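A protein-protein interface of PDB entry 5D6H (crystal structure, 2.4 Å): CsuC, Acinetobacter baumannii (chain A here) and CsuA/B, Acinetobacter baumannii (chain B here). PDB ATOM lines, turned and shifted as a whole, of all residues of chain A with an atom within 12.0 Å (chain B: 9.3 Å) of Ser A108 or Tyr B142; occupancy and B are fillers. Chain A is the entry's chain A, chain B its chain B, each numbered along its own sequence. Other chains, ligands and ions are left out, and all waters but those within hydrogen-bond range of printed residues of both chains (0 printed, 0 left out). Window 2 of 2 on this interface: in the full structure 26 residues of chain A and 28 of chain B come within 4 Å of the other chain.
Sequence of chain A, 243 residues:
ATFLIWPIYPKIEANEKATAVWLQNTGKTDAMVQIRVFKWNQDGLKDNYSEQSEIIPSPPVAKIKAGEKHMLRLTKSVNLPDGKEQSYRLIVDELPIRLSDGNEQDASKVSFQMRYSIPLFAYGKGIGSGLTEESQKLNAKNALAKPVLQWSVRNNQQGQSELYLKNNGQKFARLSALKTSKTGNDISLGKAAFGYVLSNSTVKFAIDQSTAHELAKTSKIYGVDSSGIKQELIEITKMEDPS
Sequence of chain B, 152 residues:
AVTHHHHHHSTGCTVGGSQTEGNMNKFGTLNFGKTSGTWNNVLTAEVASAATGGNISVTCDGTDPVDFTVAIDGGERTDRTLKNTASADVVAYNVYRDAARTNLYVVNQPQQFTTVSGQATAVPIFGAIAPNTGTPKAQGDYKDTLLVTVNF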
ATOM      1  N   SER A 108      -3.855 -25.108 -13.444  1.00  0.00           N
ATOM      2  CA  SER A 108      -4.129 -23.811 -14.054  1.00  0.00           C
ATOM      3  C   SER A 108      -5.629 -23.494 -14.094  1.00  0.00           C
ATOM      4  O   SER A 108      -6.281 -23.650 -15.121  1.00  0.00           O
ATOM      5  CB  SER A 108      -3.526 -23.753 -15.460  1.00  0.00           C
ATOM      6  OG  SER A 108      -3.854 -22.545 -16.127  1.00  0.00           O
ATOM      7  N   LYS A 109      -6.170 -23.031 -12.974  1.00  0.00           N
ATOM      8  CA  LYS A 109      -7.606 -22.783 -12.868  1.00  0.00           C
ATOM      9  C   LYS A 109      -7.956 -21.327 -12.537  1.00  0.00           C
ATOM     10  O   LYS A 109      -7.588 -20.824 -11.480  1.00  0.00           O
ATOM     11  CB  LYS A 109      -8.225 -23.713 -11.817  1.00  0.00           C
ATOM     12  N   VAL A 110      -8.668 -20.658 -13.441  1.00  0.00           N
ATOM     13  CA  VAL A 110      -9.212 -19.340 -13.145  1.00  0.00           C
ATOM     14  C   VAL A 110     -10.654 -19.518 -12.662  1.00  0.00           C
ATOM     15  O   VAL A 110     -11.409 -20.308 -13.231  1.00  0.00           O
ATOM     16  CB  VAL A 110      -9.124 -18.355 -14.370  1.00  0.00           C
ATOM     17  CG1 VAL A 110      -7.741 -18.385 -15.005  1.00  0.00           C
ATOM     18  CG2 VAL A 110     -10.149 -18.674 -15.424  1.00  0.00           C
ATOM     19  N   SER A 111     -11.030 -18.814 -11.597  1.00  0.00           N
ATOM     20  CA  SER A 111     -12.383 -18.933 -11.047  1.00  0.00           C
ATOM     21  C   SER A 111     -13.187 -17.647 -11.242  1.00  0.00           C
ATOM     22  O   SER A 111     -12.654 -16.643 -11.710  1.00  0.00           O
ATOM     23  CB  SER A 111     -12.323 -19.276  -9.563  1.00  0.00           C
ATOM     24  OG  SER A 111     -11.823 -18.171  -8.836  1.00  0.00           O
ATOM     25  N   PHE A 112     -14.461 -17.661 -10.864  1.00  0.00           N
ATOM     26  CA  PHE A 112     -15.311 -16.482 -11.049  1.00  0.00           C
ATOM     27  C   PHE A 112     -15.886 -15.885  -9.745  1.00  0.00           C
ATOM     28  O   PHE A 112     -16.307 -16.620  -8.852  1.00  0.00           O
ATOM     29  CB  PHE A 112     -16.428 -16.776 -12.063  1.00  0.00           C
ATOM     30  CG  PHE A 112     -15.928 -17.127 -13.449  1.00  0.00           C
ATOM     31  CD1 PHE A 112     -14.736 -16.612 -13.927  1.00  0.00           C
ATOM     32  CD2 PHE A 112     -16.658 -17.971 -14.271  1.00  0.00           C
ATOM     33  CE1 PHE A 112     -14.275 -16.918 -15.182  1.00  0.00           C
ATOM     34  CE2 PHE A 112     -16.205 -18.284 -15.538  1.00  0.00           C
ATOM     35  CZ  PHE A 112     -15.009 -17.755 -15.995  1.00  0.00           C
ATOM     36  N   THR B  29     -15.768 -23.712 -13.687  1.00  0.00           N
ATOM     37  CA  THR B  29     -14.807 -22.645 -13.979  1.00  0.00           C
ATOM     38  C   THR B  29     -14.009 -22.929 -15.256  1.00  0.00           C
ATOM     39  O   THR B  29     -14.431 -23.720 -16.103  1.00  0.00           O
ATOM     40  CB  THR B  29     -13.806 -22.444 -12.809  1.00  0.00           C
ATOM     41  OG1 THR B  29     -13.088 -23.661 -12.568  1.00  0.00           O
ATOM     42  CG2 THR B  29     -14.526 -22.026 -11.532  1.00  0.00           C
ATOM     43  N   LEU B  30     -12.854 -22.279 -15.380  1.00  0.00           N
ATOM     44  CA  LEU B  30     -11.938 -22.510 -16.500  1.00  0.00           C
ATOM     45  C   LEU B  30     -10.621 -23.155 -16.060  1.00  0.00           C
ATOM     46  O   LEU B  30      -9.796 -22.515 -15.408  1.00  0.00           O
ATOM     47  CB  LEU B  30     -11.593 -21.196 -17.190  1.00  0.00           C
ATOM     48  CG  LEU B  30     -12.440 -20.562 -18.282  1.00  0.00           C
ATOM     49  CD1 LEU B  30     -13.890 -20.435 -17.857  1.00  0.00           C
ATOM     50  CD2 LEU B  30     -11.849 -19.198 -18.590  1.00  0.00           C
ATOM     51  N   ASN B  31     -10.405 -24.408 -16.432  1.00  0.00           N
ATOM     52  CA  ASN B  31      -9.090 -25.010 -16.224  1.00  0.00           C
ATOM     53  C   ASN B  31      -8.394 -25.375 -17.534  1.00  0.00           C
ATOM     54  O   ASN B  31      -9.028 -25.848 -18.480  1.00  0.00           O
ATOM     55  CB  ASN B  31      -9.124 -26.192 -15.233  1.00  0.00           C
ATOM     56  CG  ASN B  31     -10.459 -26.911 -15.205  1.00  0.00           C
ATOM     57  OD1 ASN B  31     -11.483 -26.372 -15.624  1.00  0.00           O
ATOM     58  ND2 ASN B  31     -10.454 -28.136 -14.693  1.00  0.00           N
ATOM     59  N   PHE B  32      -7.088 -25.128 -17.584  1.00  0.00           N
ATOM     60  CA  PHE B  32      -6.315 -25.300 -18.813  1.00  0.00           C
ATOM     61  C   PHE B  32      -5.471 -26.579 -18.816  1.00  0.00           C
ATOM     62  O   PHE B  32      -4.678 -26.825 -17.904  1.00  0.00           O
ATOM     63  CB  PHE B  32      -5.430 -24.072 -19.064  1.00  0.00           C
ATOM     64  CG  PHE B  32      -6.203 -22.794 -19.283  1.00  0.00           C
ATOM     65  CD1 PHE B  32      -6.449 -22.330 -20.570  1.00  0.00           C
ATOM     66  CD2 PHE B  32      -6.676 -22.056 -18.204  1.00  0.00           C
ATOM     67  CE1 PHE B  32      -7.151 -21.159 -20.776  1.00  0.00           C
ATOM     68  CE2 PHE B  32      -7.379 -20.888 -18.402  1.00  0.00           C
ATOM     69  CZ  PHE B  32      -7.618 -20.437 -19.693  1.00  0.00           C
ATOM     70  N   LEU B  43       6.385 -24.157 -13.785  1.00  0.00           N
ATOM     71  CA  LEU B  43       7.033 -24.356 -15.088  1.00  0.00           C
ATOM     72  C   LEU B  43       7.508 -23.058 -15.738  1.00  0.00           C
ATOM     73  O   LEU B  43       7.205 -21.965 -15.259  1.00  0.00           O
ATOM     74  CB  LEU B  43       6.108 -25.119 -16.061  1.00  0.00           C
ATOM     75  CG  LEU B  43       4.712 -25.556 -15.543  1.00  0.00           C
ATOM     76  CD1 LEU B  43       3.524 -24.747 -16.097  1.00  0.00           C
ATOM     77  CD2 LEU B  43       4.470 -26.986 -15.805  1.00  0.00           C
ATOM     78  N   THR B  44       8.273 -23.198 -16.819  1.00  0.00           N
ATOM     79  CA  THR B  44       8.881 -22.065 -17.521  1.00  0.00           C
ATOM     80  C   THR B  44       9.595 -22.563 -18.781  1.00  0.00           C
ATOM     81  O   THR B  44       9.629 -21.886 -19.809  1.00  0.00           O
ATOM     82  CB  THR B  44       9.914 -21.313 -16.631  1.00  0.00           C
ATOM     83  OG1 THR B  44       9.292 -20.868 -15.416  1.00  0.00           O
ATOM     84  CG2 THR B  44      10.501 -20.106 -17.362  1.00  0.00           C
ATOM     85  N   ALA B  50      -3.231 -23.061 -25.237  1.00  0.00           N
ATOM     86  CA  ALA B  50      -4.278 -23.777 -24.488  1.00  0.00           C
ATOM     87  C   ALA B  50      -5.589 -22.985 -24.332  1.00  0.00           C
ATOM     88  O   ALA B  50      -5.570 -21.759 -24.271  1.00  0.00           O
ATOM     89  CB  ALA B  50      -3.744 -24.219 -23.115  1.00  0.00           C
ATOM     90  N   ALA B  51      -6.716 -23.697 -24.252  1.00  0.00           N
ATOM     91  CA  ALA B  51      -8.050 -23.082 -24.234  1.00  0.00           C
ATOM     92  C   ALA B  51      -9.032 -23.761 -23.260  1.00  0.00           C
ATOM     93  O   ALA B  51      -8.790 -24.884 -22.819  1.00  0.00           O
ATOM     94  CB  ALA B  51      -8.638 -23.059 -25.660  1.00  0.00           C
ATOM     95  N   THR B  52     -10.137 -23.077 -22.944  1.00  0.00           N
ATOM     96  CA  THR B  52     -11.199 -23.613 -22.070  1.00  0.00           C
ATOM     97  C   THR B  52     -12.484 -22.761 -22.079  1.00  0.00           C
ATOM     98  O   THR B  52     -12.495 -21.654 -22.611  1.00  0.00           O
ATOM     99  CB  THR B  52     -10.719 -23.777 -20.607  1.00  0.00           C
ATOM    100  N   TYR B  93      -4.682 -16.171 -19.978  1.00  0.00           N
ATOM    101  CA  TYR B  93      -4.143 -14.821 -19.862  1.00  0.00           C
ATOM    102  C   TYR B  93      -5.081 -13.789 -20.454  1.00  0.00           C
ATOM    103  O   TYR B  93      -4.838 -12.592 -20.341  1.00  0.00           O
ATOM    104  CB  TYR B  93      -2.767 -14.718 -20.517  1.00  0.00           C
ATOM    105  CG  TYR B  93      -1.668 -15.206 -19.621  1.00  0.00           C
ATOM    106  CD1 TYR B  93      -0.708 -14.336 -19.119  1.00  0.00           C
ATOM    107  CD2 TYR B  93      -1.612 -16.540 -19.242  1.00  0.00           C
ATOM    108  CE1 TYR B  93       0.290 -14.794 -18.282  1.00  0.00           C
ATOM    109  CE2 TYR B  93      -0.626 -17.004 -18.414  1.00  0.00           C
ATOM    110  CZ  TYR B  93       0.324 -16.135 -17.932  1.00  0.00           C
ATOM    111  OH  TYR B  93       1.309 -16.628 -17.100  1.00  0.00           O
ATOM    112  N   ALA B 128      -7.816 -18.429 -22.931  1.00  0.00           N
ATOM    113  CA  ALA B 128      -6.737 -18.786 -23.840  1.00  0.00           C
ATOM    114  C   ALA B 128      -5.375 -18.373 -23.319  1.00  0.00           C
ATOM    115  O   ALA B 128      -5.246 -17.427 -22.538  1.00  0.00           O
ATOM    116  CB  ALA B 128      -6.970 -18.169 -25.219  1.00  0.00           C
ATOM    117  N   ILE B 129      -4.359 -19.101 -23.767  1.00  0.00           N
ATOM    118  CA  ILE B 129      -2.975 -18.697 -23.568  1.00  0.00           C
ATOM    119  C   ILE B 129      -2.124 -19.075 -24.779  1.00  0.00           C
ATOM    120  O   ILE B 129      -2.597 -19.741 -25.694  1.00  0.00           O
ATOM    121  CB  ILE B 129      -2.376 -19.288 -22.278  1.00  0.00           C
ATOM    122  CG1 ILE B 129      -0.926 -18.819 -22.115  1.00  0.00           C
ATOM    123  CG2 ILE B 129      -2.460 -20.808 -22.296  1.00  0.00           C
ATOM    124  CD1 ILE B 129      -0.713 -17.327 -22.374  1.00  0.00           C
ATOM    125  N   THR B 135      -3.291 -12.700 -15.985  1.00  0.00           N
ATOM    126  CA  THR B 135      -1.985 -12.610 -15.326  1.00  0.00           C
ATOM    127  C   THR B 135      -1.858 -13.530 -14.111  1.00  0.00           C
ATOM    128  O   THR B 135      -1.590 -13.061 -13.001  1.00  0.00           O
ATOM    129  CB  THR B 135      -1.680 -11.171 -14.867  1.00  0.00           C
ATOM    130  N   PRO B 136      -2.027 -14.846 -14.326  1.00  0.00           N
ATOM    131  CA  PRO B 136      -2.038 -15.905 -13.306  1.00  0.00           C
ATOM    132  C   PRO B 136      -0.769 -15.930 -12.456  1.00  0.00           C
ATOM    133  O   PRO B 136       0.158 -15.159 -12.704  1.00  0.00           O
ATOM    134  CB  PRO B 136      -2.147 -17.185 -14.139  1.00  0.00           C
ATOM    135  N   LYS B 137      -0.735 -16.812 -11.461  1.00  0.00           N
ATOM    136  CA  LYS B 137       0.397 -16.889 -10.534  1.00  0.00           C
ATOM    137  C   LYS B 137       0.362 -18.164  -9.713  1.00  0.00           C
ATOM    138  O   LYS B 137      -0.708 -18.583  -9.266  1.00  0.00           O
ATOM    139  CB  LYS B 137       0.425 -15.671  -9.595  1.00  0.00           C
ATOM    140  CG  LYS B 137       1.415 -15.796  -8.438  1.00  0.00           C
ATOM    141  CD  LYS B 137       1.712 -14.462  -7.763  1.00  0.00           C
ATOM    142  CE  LYS B 137       2.468 -13.511  -8.683  1.00  0.00           C
ATOM    143  NZ  LYS B 137       2.648 -12.161  -8.060  1.00  0.00           N
ATOM    144  N   ALA B 138       1.536 -18.775  -9.538  1.00  0.00           N
ATOM    145  CA  ALA B 138       1.735 -19.879  -8.596  1.00  0.00           C
ATOM    146  C   ALA B 138       3.221 -20.029  -8.238  1.00  0.00           C
ATOM    147  O   ALA B 138       3.780 -21.136  -8.227  1.00  0.00           O
ATOM    148  CB  ALA B 138       1.184 -21.175  -9.165  1.00  0.00           C
ATOM    149  N   TYR B 142      -1.538 -22.808 -11.114  1.00  0.00           N
ATOM    150  CA  TYR B 142      -1.669 -21.363 -11.299  1.00  0.00           C
ATOM    151  C   TYR B 142      -3.133 -20.943 -11.288  1.00  0.00           C
ATOM    152  O   TYR B 142      -3.925 -21.420 -12.090  1.00  0.00           O
ATOM    153  CB  TYR B 142      -1.031 -20.924 -12.613  1.00  0.00           C
ATOM    154  CG  TYR B 142       0.449 -21.206 -12.728  1.00  0.00           C
ATOM    155  CD1 TYR B 142       1.356 -20.172 -12.916  1.00  0.00           C
ATOM    156  CD2 TYR B 142       0.940 -22.508 -12.670  1.00  0.00           C
ATOM    157  CE1 TYR B 142       2.706 -20.425 -13.036  1.00  0.00           C
ATOM    158  CE2 TYR B 142       2.284 -22.771 -12.786  1.00  0.00           C
ATOM    159  CZ  TYR B 142       3.167 -21.728 -12.966  1.00  0.00           C
ATOM    160  OH  TYR B 142       4.515 -21.987 -13.089  1.00  0.00           O
ATOM    161  N   LYS B 143      -3.491 -20.045 -10.382  1.00  0.00           N
ATOM    162  CA  LYS B 143      -4.876 -19.622 -10.260  1.00  0.00           C
ATOM    163  C   LYS B 143      -5.030 -18.133 -10.519  1.00  0.00           C
ATOM    164  O   LYS B 143      -4.181 -17.326 -10.140  1.00  0.00           O
ATOM    165  CB  LYS B 143      -5.418 -19.939  -8.862  1.00  0.00           C
ATOM    166  CG  LYS B 143      -5.090 -21.329  -8.333  1.00  0.00           C
ATOM    167  CD  LYS B 143      -5.636 -22.438  -9.228  1.00  0.00           C
ATOM    168  CE  LYS B 143      -5.316 -23.813  -8.654  1.00  0.00           C
ATOM    169  NZ  LYS B 143      -5.813 -23.961  -7.247  1.00  0.00           N
ATOM    170  N   ASP B 144      -6.123 -17.765 -11.175  1.00  0.00           N
ATOM    171  CA  ASP B 144      -6.527 -16.370 -11.186  1.00  0.00           C
ATOM    172  C   ASP B 144      -7.955 -16.220 -10.682  1.00  0.00           C
ATOM    173  O   ASP B 144      -8.786 -17.118 -10.838  1.00  0.00           O
ATOM    174  CB  ASP B 144      -6.368 -15.737 -12.568  1.00  0.00           C
ATOM    175  CG  ASP B 144      -6.444 -14.221 -12.515  1.00  0.00           C
ATOM    176  OD1 ASP B 144      -6.330 -13.682 -11.395  1.00  0.00           O
ATOM    177  OD2 ASP B 144      -6.609 -13.570 -13.573  1.00  0.00           O
ATOM    178  N   THR B 145      -8.223 -15.081 -10.058  1.00  0.00           N
ATOM    179  CA  THR B 145      -9.574 -14.711  -9.666  1.00  0.00           C
ATOM    180  C   THR B 145     -10.038 -13.465 -10.443  1.00  0.00           C
ATOM    181  O   THR B 145      -9.545 -12.358 -10.226  1.00  0.00           O
ATOM    182  CB  THR B 145      -9.649 -14.468  -8.150  1.00  0.00           C
ATOM    183  OG1 THR B 145      -9.417 -15.704  -7.449  1.00  0.00           O
ATOM    184  CG2 THR B 145     -11.008 -13.902  -7.756  1.00  0.00           C
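O of Ser A108 lies within hydrogen-bond range of N of Phe B32, at 3.0 Å. The backbone NH (N) of Lys A109 is in hydrogen-bond range of the backbone carbonyl oxygen (O) of Tyr B142. The backbone NH (N) of Asp B144 lies within hydrogen-bond range of the backbone carbonyl oxygen (O) of Lys A109 (3.4 Å). The backbone NH (N) of Val A110 sits at hydrogen-bond distance from the backbone carbonyl oxygen (O) of Leu B30. The backbone NH of Ser A111 is in hydrogen-bond range of the backbone carbonyl oxygen of Asp B144, at 2.9 Å.
The backbone NH (N) of Leu B43 is in hydrogen-bond range of the side-chain hydroxyl (OH) of Tyr B142, at 2.9 Å. The backbone NH (N) of Lys B143 sits at hydrogen-bond distance from the backbone carbonyl oxygen (O) of Lys B137 (3.3 Å).
Ser A108 touches Leu B30. Asn B31 touches Ser A108 (CA to O, 3.3 Å). Ser A108 touches Tyr B142 (CA to O, 3.1 Å). CA of Lys A109 touches O of Leu B30 (3.4 Å). O of Lys A109 touches CA of Lys B143 (3.2 Å). Val A110 touches Thr B29. CA of Val A110 touches O of Asp B144 (3.2 Å). Ser A111 touches Thr B29 (CA to CG2, 3.8 Å). Thr B145 touches Ser A111. Leu B30 touches Phe A112 (CD1 to CZ, 3.4 Å).
Of chain A, only Ser A108 (3.1 Å) and Lys A109 (2.9 Å) come within 4 Å of Tyr B142. Lys A109 touches just these residues of chain B: Leu B30 (3.4 Å), Tyr B142 (2.9 Å), Lys B143 (3.2 Å) and Asp B144 (3.4 Å). Leu B43 touches none of the printed residues of chain A. No residue of chain A comes within 4 Å of Pro B136. No residue of chain A comes within 4 Å of Ala B138. Of chain A, only Lys A109 (3.2 Å) comes within 4 Å of Lys B143. Of the printed residues of chain A, Asp B144 touches Lys A109 (3.4 Å), Val A110 (3.2 Å) and Ser A111 (2.9 Å). Of the printed residues of chain B, Ser A111 touches Thr B29 (3.8 Å), Asp B144 (2.9 Å) and Thr B145 (3.7 Å). Printed residues of chain A within 4 Å of Leu B30: Ser A108, Lys A109, Val A110 and Phe A112. The nearest residue of chain B that does not touch Ser A108 is Lys B143 (5.0 Å). The nearest residue of chain A that does not touch Tyr B142 is Val A110 (5.0 Å).
Hydrophobic or aromatic side chains of chain B that line the printed part of chain A: Leu B30 and Phe B32. Hydrophobic or aromatic side chains of chain A that line the printed part of chain B: Val A110 and Phe A112.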
